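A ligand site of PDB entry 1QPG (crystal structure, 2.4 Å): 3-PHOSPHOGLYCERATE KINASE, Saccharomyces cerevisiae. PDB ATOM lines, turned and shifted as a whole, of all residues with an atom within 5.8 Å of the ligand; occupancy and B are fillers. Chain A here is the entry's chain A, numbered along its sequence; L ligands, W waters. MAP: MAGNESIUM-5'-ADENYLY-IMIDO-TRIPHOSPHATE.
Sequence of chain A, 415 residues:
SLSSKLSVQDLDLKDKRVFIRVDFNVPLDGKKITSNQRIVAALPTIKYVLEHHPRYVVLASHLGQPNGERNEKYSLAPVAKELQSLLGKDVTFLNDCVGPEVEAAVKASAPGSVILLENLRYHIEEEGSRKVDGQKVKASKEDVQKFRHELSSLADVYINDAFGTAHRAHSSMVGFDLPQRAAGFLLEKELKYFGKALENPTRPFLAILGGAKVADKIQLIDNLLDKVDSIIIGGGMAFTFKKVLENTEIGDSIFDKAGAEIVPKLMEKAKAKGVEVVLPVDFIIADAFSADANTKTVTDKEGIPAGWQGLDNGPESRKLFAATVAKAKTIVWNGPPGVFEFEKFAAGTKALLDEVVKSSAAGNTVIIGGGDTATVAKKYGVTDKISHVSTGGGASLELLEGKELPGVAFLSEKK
OG1 of Thr 373 sits at hydrogen-bond distance from O2B of the ligand (2.6 Å). A nitrogen (N3B) of the ligand is in hydrogen-bond range of the side-chain amide oxygen (OD1) of Asn 334, 2.8 Å away. N of Thr 373 is in hydrogen-bond range of O2B of the ligand (2.9 Å). N of Asp 372 lies within hydrogen-bond range of O2B of the ligand (3.3 Å). O2' of the ligand sits at hydrogen-bond distance from OE2 of Glu 341 (2.8 Å). N of Phe 340 sits at hydrogen-bond distance from O2' of the ligand (3.4 Å). The backbone NH (N) of Gly 236 lies close to a nitrogen (N7) of the ligand (3.4 Å). The backbone carbonyl oxygen (O) of Gly 338 lies within hydrogen-bond range of an oxygen (O2') of the ligand (3.1 Å). O2G of the ligand lies within hydrogen-bond range of N of Gly 371 (2.7 Å). The side-chain amino group (NZ) of Lys 217 is in salt-bridge range of an oxygen (O3G) of the ligand, at 3.9 Å. A nitrogen (N6) of the ligand sits at hydrogen-bond distance from the backbone carbonyl oxygen (O) of Gly 310, 3.3 Å away.
OG1 of Thr 373 lies within hydrogen-bond range of N of Gly 335. N of Gly 235 sits at hydrogen-bond distance from O of Pro 337, 3.2 Å away. The side-chain amino group of Lys 217 sits at hydrogen-bond distance from the side-chain amide oxygen of Asn 334, 3.0 Å away. The backbone NH (N) of Val 339 sits at hydrogen-bond distance from the backbone carbonyl oxygen (O) of Leu 311 (2.9 Å). The backbone carbonyl oxygen (O) of Pro 336 is in hydrogen-bond range of the backbone NH (N) of Gly 211 (3.3 Å). The backbone carbonyl oxygen of Gly 211 is in hydrogen-bond range of the backbone NH of Gly 236 (2.6 Å). The side-chain amide nitrogen of Asn 334 sits at hydrogen-bond distance from the backbone carbonyl oxygen of Gly 369. O of Asn 334 sits at hydrogen-bond distance from N of Gly 210 (3.1 Å).
Water W2 lies within hydrogen-bond range of a nitrogen (N6) of the ligand, the backbone carbonyl oxygen (O) of Pro 337, the backbone NH (N) of Asp 312 and the backbone carbonyl oxygen (O) of Leu 311. Water W1 lies within hydrogen-bond range of O1A of the ligand (2.9 Å), N of Lys 213 (2.9 Å) and N of Ala 212 (3.1 Å).
CA of Gly 211 touches O1A of the ligand, 3.7 Å away. Ala 212 touches the ligand (N to O1A, 3.7 Å). Gly 235 touches the ligand (CA to N7, 3.5 Å). CE2 of Phe 239 touches N6 of the ligand (3.6 Å). Ile 254 touches the ligand. Leu 311 touches the ligand (CA to N6, 3.97 Å). N of Gly 335 touches O2B of the ligand (3.7 Å). Pro 336 touches the ligand. C of Pro 337 touches N7 of the ligand (3.9 Å). CA of Val 339 touches O2' of the ligand (3.0 Å). Gly 370 touches the ligand (CA to O2G, 3.6 Å). Hydrophobic or aromatic side chains within 4 Å of the ligand: Phe 239, Ile 254, Pro 336, Val 339 and Phe 340. Of the 28 residues printed, 21 come within 4 Å of the ligand. The nearest printed residue that does not touch the ligand is Gly 210 (4.4 Å).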
ATOM      1  N   GLY A 210     -12.756  28.902  -7.366  1.00  0.00           N
ATOM      2  CA  GLY A 210     -14.015  28.273  -7.735  1.00  0.00           C
ATOM      3  C   GLY A 210     -15.153  28.931  -6.987  1.00  0.00           C
ATOM      4  O   GLY A 210     -14.998  30.036  -6.489  1.00  0.00           O
ATOM      5  N   GLY A 211     -16.310  28.277  -6.905  1.00  0.00           N
ATOM      6  CA  GLY A 211     -17.422  28.850  -6.181  1.00  0.00           C
ATOM      7  C   GLY A 211     -18.504  29.372  -7.082  1.00  0.00           C
ATOM      8  O   GLY A 211     -18.554  29.020  -8.259  1.00  0.00           O
ATOM      9  N   ALA A 212     -19.334  30.266  -6.542  1.00  0.00           N
ATOM     10  CA  ALA A 212     -20.453  30.838  -7.268  1.00  0.00           C
ATOM     11  C   ALA A 212     -20.251  32.063  -8.177  1.00  0.00           C
ATOM     12  O   ALA A 212     -20.388  31.953  -9.401  1.00  0.00           O
ATOM     13  CB  ALA A 212     -21.613  31.086  -6.302  1.00  0.00           C
ATOM     14  N   LYS A 213     -19.953  33.232  -7.614  1.00  0.00           N
ATOM     15  CA  LYS A 213     -19.807  34.443  -8.414  1.00  0.00           C
ATOM     16  C   LYS A 213     -18.382  34.895  -8.716  1.00  0.00           C
ATOM     17  O   LYS A 213     -17.499  34.836  -7.868  1.00  0.00           O
ATOM     18  CB  LYS A 213     -20.571  35.612  -7.779  1.00  0.00           C
ATOM     19  CG  LYS A 213     -22.070  35.397  -7.617  1.00  0.00           C
ATOM     20  CD  LYS A 213     -22.804  35.340  -8.963  1.00  0.00           C
ATOM     21  CE  LYS A 213     -24.305  35.021  -8.770  1.00  0.00           C
ATOM     22  NZ  LYS A 213     -25.101  35.094 -10.029  1.00  0.00           N
ATOM     23  N   LYS A 217     -14.734  37.938  -6.855  1.00  0.00           N
ATOM     24  CA  LYS A 217     -13.321  37.612  -6.943  1.00  0.00           C
ATOM     25  C   LYS A 217     -12.558  38.313  -8.052  1.00  0.00           C
ATOM     26  O   LYS A 217     -11.438  37.915  -8.382  1.00  0.00           O
ATOM     27  CB  LYS A 217     -13.143  36.101  -7.005  1.00  0.00           C
ATOM     28  CG  LYS A 217     -14.159  35.340  -6.152  1.00  0.00           C
ATOM     29  CD  LYS A 217     -13.640  34.030  -5.596  1.00  0.00           C
ATOM     30  CE  LYS A 217     -14.669  33.419  -4.665  1.00  0.00           C
ATOM     31  NZ  LYS A 217     -14.100  32.292  -3.877  1.00  0.00           N
ATOM     32  N   GLY A 235     -15.865  25.579 -10.694  1.00  0.00           N
ATOM     33  CA  GLY A 235     -17.124  25.924 -10.066  1.00  0.00           C
ATOM     34  C   GLY A 235     -18.087  26.725 -10.897  1.00  0.00           C
ATOM     35  O   GLY A 235     -18.023  26.727 -12.117  1.00  0.00           O
ATOM     36  N   GLY A 236     -19.009  27.412 -10.222  1.00  0.00           N
ATOM     37  CA  GLY A 236     -19.998  28.218 -10.901  1.00  0.00           C
ATOM     38  C   GLY A 236     -19.353  29.458 -11.481  1.00  0.00           C
ATOM     39  O   GLY A 236     -20.000  30.240 -12.166  1.00  0.00           O
ATOM     40  N   MET A 237     -18.071  29.641 -11.182  1.00  0.00           N
ATOM     41  CA  MET A 237     -17.318  30.774 -11.672  1.00  0.00           C
ATOM     42  C   MET A 237     -16.989  30.620 -13.157  1.00  0.00           C
ATOM     43  O   MET A 237     -17.203  31.535 -13.959  1.00  0.00           O
ATOM     44  CB  MET A 237     -16.038  30.909 -10.853  1.00  0.00           C
ATOM     45  CG  MET A 237     -15.223  32.118 -11.151  1.00  0.00           C
ATOM     46  SD  MET A 237     -14.149  32.449  -9.753  1.00  0.00           S
ATOM     47  CE  MET A 237     -12.534  32.315 -10.502  1.00  0.00           C
ATOM     48  N   PHE A 239     -18.437  29.242 -15.676  1.00  0.00           N
ATOM     49  CA  PHE A 239     -19.450  29.469 -16.679  1.00  0.00           C
ATOM     50  C   PHE A 239     -19.382  30.845 -17.329  1.00  0.00           C
ATOM     51  O   PHE A 239     -19.645  30.981 -18.524  1.00  0.00           O
ATOM     52  CB  PHE A 239     -20.823  29.154 -16.100  1.00  0.00           C
ATOM     53  CG  PHE A 239     -20.924  27.744 -15.600  1.00  0.00           C
ATOM     54  CD1 PHE A 239     -21.086  26.701 -16.490  1.00  0.00           C
ATOM     55  CD2 PHE A 239     -20.708  27.462 -14.262  1.00  0.00           C
ATOM     56  CE1 PHE A 239     -21.012  25.398 -16.054  1.00  0.00           C
ATOM     57  CE2 PHE A 239     -20.641  26.163 -13.821  1.00  0.00           C
ATOM     58  CZ  PHE A 239     -20.787  25.133 -14.721  1.00  0.00           C
ATOM     59  N   ILE A 254     -24.657  29.430 -13.522  1.00  0.00           N
ATOM     60  CA  ILE A 254     -24.320  30.712 -12.930  1.00  0.00           C
ATOM     61  C   ILE A 254     -23.614  31.627 -13.924  1.00  0.00           C
ATOM     62  O   ILE A 254     -22.559  31.274 -14.462  1.00  0.00           O
ATOM     63  CB  ILE A 254     -23.419  30.540 -11.689  1.00  0.00           C
ATOM     64  CG1 ILE A 254     -24.197  29.822 -10.585  1.00  0.00           C
ATOM     65  CG2 ILE A 254     -22.933  31.890 -11.183  1.00  0.00           C
ATOM     66  CD1 ILE A 254     -25.514  30.498 -10.235  1.00  0.00           C
ATOM     67  N   GLY A 310     -24.964  23.050 -15.225  1.00  0.00           N
ATOM     68  CA  GLY A 310     -23.836  22.276 -14.748  1.00  0.00           C
ATOM     69  C   GLY A 310     -23.608  22.476 -13.266  1.00  0.00           C
ATOM     70  O   GLY A 310     -23.473  23.602 -12.813  1.00  0.00           O
ATOM     71  N   LEU A 311     -23.547  21.382 -12.516  1.00  0.00           N
ATOM     72  CA  LEU A 311     -23.353  21.483 -11.089  1.00  0.00           C
ATOM     73  C   LEU A 311     -22.067  20.876 -10.600  1.00  0.00           C
ATOM     74  O   LEU A 311     -21.786  20.900  -9.408  1.00  0.00           O
ATOM     75  CB  LEU A 311     -24.564  20.931 -10.345  1.00  0.00           C
ATOM     76  CG  LEU A 311     -25.891  21.574 -10.767  1.00  0.00           C
ATOM     77  CD1 LEU A 311     -27.042  21.014  -9.992  1.00  0.00           C
ATOM     78  CD2 LEU A 311     -25.846  23.061 -10.569  1.00  0.00           C
ATOM     79  N   ASP A 312     -21.262  20.341 -11.513  1.00  0.00           N
ATOM     80  CA  ASP A 312     -19.980  19.746 -11.117  1.00  0.00           C
ATOM     81  C   ASP A 312     -19.051  19.578 -12.321  1.00  0.00           C
ATOM     82  O   ASP A 312     -19.449  19.728 -13.483  1.00  0.00           O
ATOM     83  CB  ASP A 312     -20.179  18.409 -10.375  1.00  0.00           C
ATOM     84  CG  ASP A 312     -18.866  17.829  -9.818  1.00  0.00           C
ATOM     85  OD1 ASP A 312     -17.941  18.572  -9.433  1.00  0.00           O
ATOM     86  OD2 ASP A 312     -18.751  16.581  -9.758  1.00  0.00           O
ATOM     87  N   ASN A 334      -9.161  28.378  -3.077  1.00  0.00           N
ATOM     88  CA  ASN A 334     -10.342  28.999  -2.509  1.00  0.00           C
ATOM     89  C   ASN A 334     -11.507  28.775  -3.474  1.00  0.00           C
ATOM     90  O   ASN A 334     -11.516  29.305  -4.573  1.00  0.00           O
ATOM     91  CB  ASN A 334     -10.113  30.509  -2.289  1.00  0.00           C
ATOM     92  CG  ASN A 334     -11.394  31.238  -1.840  1.00  0.00           C
ATOM     93  OD1 ASN A 334     -12.477  30.679  -1.875  1.00  0.00           O
ATOM     94  ND2 ASN A 334     -11.256  32.495  -1.442  1.00  0.00           N
ATOM     95  N   GLY A 335     -12.486  27.985  -3.025  1.00  0.00           N
ATOM     96  CA  GLY A 335     -13.672  27.689  -3.821  1.00  0.00           C
ATOM     97  C   GLY A 335     -13.755  26.253  -4.330  1.00  0.00           C
ATOM     98  O   GLY A 335     -12.788  25.740  -4.903  1.00  0.00           O
ATOM     99  N   PRO A 336     -14.886  25.558  -4.098  1.00  0.00           N
ATOM    100  CA  PRO A 336     -15.102  24.176  -4.549  1.00  0.00           C
ATOM    101  C   PRO A 336     -15.430  24.116  -6.063  1.00  0.00           C
ATOM    102  O   PRO A 336     -16.144  24.975  -6.563  1.00  0.00           O
ATOM    103  CB  PRO A 336     -16.310  23.728  -3.703  1.00  0.00           C
ATOM    104  CG  PRO A 336     -16.282  24.637  -2.511  1.00  0.00           C
ATOM    105  CD  PRO A 336     -15.942  25.959  -3.144  1.00  0.00           C
ATOM    106  N   PRO A 337     -14.930  23.091  -6.786  1.00  0.00           N
ATOM    107  CA  PRO A 337     -15.192  22.959  -8.241  1.00  0.00           C
ATOM    108  C   PRO A 337     -16.633  22.619  -8.600  1.00  0.00           C
ATOM    109  O   PRO A 337     -17.013  22.693  -9.766  1.00  0.00           O
ATOM    110  CB  PRO A 337     -14.262  21.824  -8.658  1.00  0.00           C
ATOM    111  CG  PRO A 337     -13.207  21.827  -7.609  1.00  0.00           C
ATOM    112  CD  PRO A 337     -13.964  22.066  -6.348  1.00  0.00           C
ATOM    113  N   GLY A 338     -17.439  22.215  -7.602  1.00  0.00           N
ATOM    114  CA  GLY A 338     -18.830  21.875  -7.873  1.00  0.00           C
ATOM    115  C   GLY A 338     -19.698  21.891  -6.623  1.00  0.00           C
ATOM    116  O   GLY A 338     -19.180  22.010  -5.514  1.00  0.00           O
ATOM    117  N   VAL A 339     -21.015  21.786  -6.809  1.00  0.00           N
ATOM    118  CA  VAL A 339     -21.982  21.776  -5.712  1.00  0.00           C
ATOM    119  C   VAL A 339     -21.787  20.486  -4.909  1.00  0.00           C
ATOM    120  O   VAL A 339     -22.567  19.531  -5.019  1.00  0.00           O
ATOM    121  CB  VAL A 339     -23.420  21.841  -6.253  1.00  0.00           C
ATOM    122  CG1 VAL A 339     -24.421  21.850  -5.143  1.00  0.00           C
ATOM    123  CG2 VAL A 339     -23.572  23.071  -7.077  1.00  0.00           C
ATOM    124  N   PHE A 340     -20.745  20.487  -4.069  1.00  0.00           N
ATOM    125  CA  PHE A 340     -20.387  19.325  -3.271  1.00  0.00           C
ATOM    126  C   PHE A 340     -21.359  18.951  -2.145  1.00  0.00           C
ATOM    127  O   PHE A 340     -21.234  17.869  -1.548  1.00  0.00           O
ATOM    128  CB  PHE A 340     -18.953  19.471  -2.750  1.00  0.00           C
ATOM    129  CG  PHE A 340     -18.830  20.417  -1.597  1.00  0.00           C
ATOM    130  CD1 PHE A 340     -19.139  21.757  -1.737  1.00  0.00           C
ATOM    131  CD2 PHE A 340     -18.450  19.947  -0.347  1.00  0.00           C
ATOM    132  CE1 PHE A 340     -19.092  22.606  -0.659  1.00  0.00           C
ATOM    133  CE2 PHE A 340     -18.410  20.800   0.736  1.00  0.00           C
ATOM    134  CZ  PHE A 340     -18.728  22.128   0.577  1.00  0.00           C
ATOM    135  N   GLU A 341     -22.313  19.840  -1.849  1.00  0.00           N
ATOM    136  CA  GLU A 341     -23.312  19.582  -0.806  1.00  0.00           C
ATOM    137  C   GLU A 341     -24.151  18.355  -1.160  1.00  0.00           C
ATOM    138  O   GLU A 341     -24.718  17.698  -0.280  1.00  0.00           O
ATOM    139  CB  GLU A 341     -24.256  20.778  -0.617  1.00  0.00           C
ATOM    140  CG  GLU A 341     -23.589  22.068  -0.154  1.00  0.00           C
ATOM    141  CD  GLU A 341     -23.070  22.919  -1.291  1.00  0.00           C
ATOM    142  OE1 GLU A 341     -23.861  23.298  -2.182  1.00  0.00           O
ATOM    143  OE2 GLU A 341     -21.869  23.219  -1.305  1.00  0.00           O
ATOM    144  N   GLY A 369      -8.013  28.597   1.733  1.00  0.00           N
ATOM    145  CA  GLY A 369      -8.489  29.856   2.224  1.00  0.00           C
ATOM    146  C   GLY A 369      -9.872  30.123   1.731  1.00  0.00           C
ATOM    147  O   GLY A 369     -10.093  31.059   0.959  1.00  0.00           O
ATOM    148  N   GLY A 370     -10.822  29.288   2.145  1.00  0.00           N
ATOM    149  CA  GLY A 370     -12.196  29.462   1.749  1.00  0.00           C
ATOM    150  C   GLY A 370     -13.085  28.906   2.843  1.00  0.00           C
ATOM    151  O   GLY A 370     -12.648  28.037   3.605  1.00  0.00           O
ATOM    152  N   GLY A 371     -14.297  29.418   2.965  1.00  0.00           N
ATOM    153  CA  GLY A 371     -15.202  28.919   3.988  1.00  0.00           C
ATOM    154  C   GLY A 371     -15.541  27.470   3.714  1.00  0.00           C
ATOM    155  O   GLY A 371     -15.086  26.557   4.424  1.00  0.00           O
ATOM    156  N   ASP A 372     -16.280  27.244   2.628  1.00  0.00           N
ATOM    157  CA  ASP A 372     -16.697  25.910   2.221  1.00  0.00           C
ATOM    158  C   ASP A 372     -15.502  25.050   1.810  1.00  0.00           C
ATOM    159  O   ASP A 372     -15.562  23.818   1.881  1.00  0.00           O
ATOM    160  CB  ASP A 372     -17.720  25.989   1.106  1.00  0.00           C
ATOM    161  CG  ASP A 372     -19.030  26.579   1.579  1.00  0.00           C
ATOM    162  OD1 ASP A 372     -19.694  25.936   2.428  1.00  0.00           O
ATOM    163  OD2 ASP A 372     -19.405  27.690   1.130  1.00  0.00           O
ATOM    164  N   THR A 373     -14.414  25.691   1.374  1.00  0.00           N
ATOM    165  CA  THR A 373     -13.224  24.956   0.998  1.00  0.00           C
ATOM    166  C   THR A 373     -12.566  24.303   2.217  1.00  0.00           C
ATOM    167  O   THR A 373     -11.852  23.307   2.090  1.00  0.00           O
ATOM    168  CB  THR A 373     -12.209  25.829   0.275  1.00  0.00           C
ATOM    169  OG1 THR A 373     -12.862  26.534  -0.773  1.00  0.00           O
ATOM    170  CG2 THR A 373     -11.143  24.981  -0.326  1.00  0.00           C
ATOM    171  N   ALA A 374     -12.796  24.879   3.406  1.00  0.00           N
ATOM    172  CA  ALA A 374     -12.264  24.312   4.644  1.00  0.00           C
ATOM    173  C   ALA A 374     -13.229  23.212   5.100  1.00  0.00           C
ATOM    174  O   ALA A 374     -12.803  22.139   5.528  1.00  0.00           O
ATOM    175  CB  ALA A 374     -12.120  25.372   5.705  1.00  0.00           C
ATOM    176  N   LEU A 397      -9.102  37.113   2.222  1.00  0.00           N
ATOM    177  CA  LEU A 397      -9.431  37.584   0.888  1.00  0.00           C
ATOM    178  C   LEU A 397      -8.682  38.882   0.592  1.00  0.00           C
ATOM    179  O   LEU A 397      -7.879  38.962  -0.352  1.00  0.00           O
ATOM    180  CB  LEU A 397     -10.939  37.832   0.759  1.00  0.00           C
ATOM    181  CG  LEU A 397     -11.424  38.320  -0.613  1.00  0.00           C
ATOM    182  CD1 LEU A 397     -11.194  37.225  -1.666  1.00  0.00           C
ATOM    183  CD2 LEU A 397     -12.895  38.762  -0.574  1.00  0.00           C
HETATM  184  PG  MAP L   1     -15.160  32.263   0.473  1.00  0.00           P
HETATM  185  O1G MAP L   1     -16.552  32.782   0.379  1.00  0.00           O
HETATM  186  O2G MAP L   1     -14.792  31.895   1.884  1.00  0.00           O
HETATM  187  O3G MAP L   1     -14.214  33.282  -0.072  1.00  0.00           O
HETATM  188  PB  MAP L   1     -15.847  29.200  -0.381  1.00  0.00           P
HETATM  189  O1B MAP L   1     -16.581  29.325   0.917  1.00  0.00           O
HETATM  190  O2B MAP L   1     -14.928  28.031  -0.284  1.00  0.00           O
HETATM  191  N3B MAP L   1     -14.881  30.688  -0.509  1.00  0.00           N
HETATM  192  PA  MAP L   1     -17.973  30.048  -2.088  1.00  0.00           P
HETATM  193  O1A MAP L   1     -17.824  30.970  -3.222  1.00  0.00           O
HETATM  194  O2A MAP L   1     -18.905  30.630  -1.086  1.00  0.00           O
HETATM  195  O3A MAP L   1     -16.779  29.211  -1.599  1.00  0.00           O
HETATM  196  O5' MAP L   1     -18.971  28.958  -2.725  1.00  0.00           O
HETATM  197  C5' MAP L   1     -19.157  27.572  -2.420  1.00  0.00           C
HETATM  198  C4' MAP L   1     -20.607  27.316  -2.827  1.00  0.00           C
HETATM  199  O4' MAP L   1     -20.636  27.490  -4.252  1.00  0.00           O
HETATM  200  C3' MAP L   1     -21.142  25.922  -2.612  1.00  0.00           C
HETATM  201  O3' MAP L   1     -22.587  25.788  -2.833  1.00  0.00           O
HETATM  202  C2' MAP L   1     -20.444  25.262  -3.811  1.00  0.00           C
HETATM  203  O2' MAP L   1     -20.962  23.918  -3.906  1.00  0.00           O
HETATM  204  C1' MAP L   1     -21.105  26.229  -4.776  1.00  0.00           C
HETATM  205  N9  MAP L   1     -20.693  25.953  -6.192  1.00  0.00           N
HETATM  206  C8  MAP L   1     -19.628  25.250  -6.711  1.00  0.00           C
HETATM  207  N7  MAP L   1     -19.749  24.943  -7.970  1.00  0.00           N
HETATM  208  C5  MAP L   1     -20.980  25.507  -8.305  1.00  0.00           C
HETATM  209  C6  MAP L   1     -21.710  25.508  -9.504  1.00  0.00           C
HETATM  210  N6  MAP L   1     -21.306  24.845 -10.587  1.00  0.00           N
HETATM  211  N1  MAP L   1     -22.870  26.166  -9.518  1.00  0.00           N
HETATM  212  C2  MAP L   1     -23.301  26.753  -8.385  1.00  0.00           C
HETATM  213  N3  MAP L   1     -22.716  26.794  -7.193  1.00  0.00           N
HETATM  214  C4  MAP L   1     -21.537  26.147  -7.240  1.00  0.00           C
HETATM  215 MG   MAP L   1     -18.233  31.146   0.939  1.00  0.00          MG
HETATM  216  O   HOH W   1     -18.479  32.963  -5.170  1.00  0.00           O
HETATM  217  O   HOH W   2     -19.455  23.075 -10.802  1.00  0.00           O
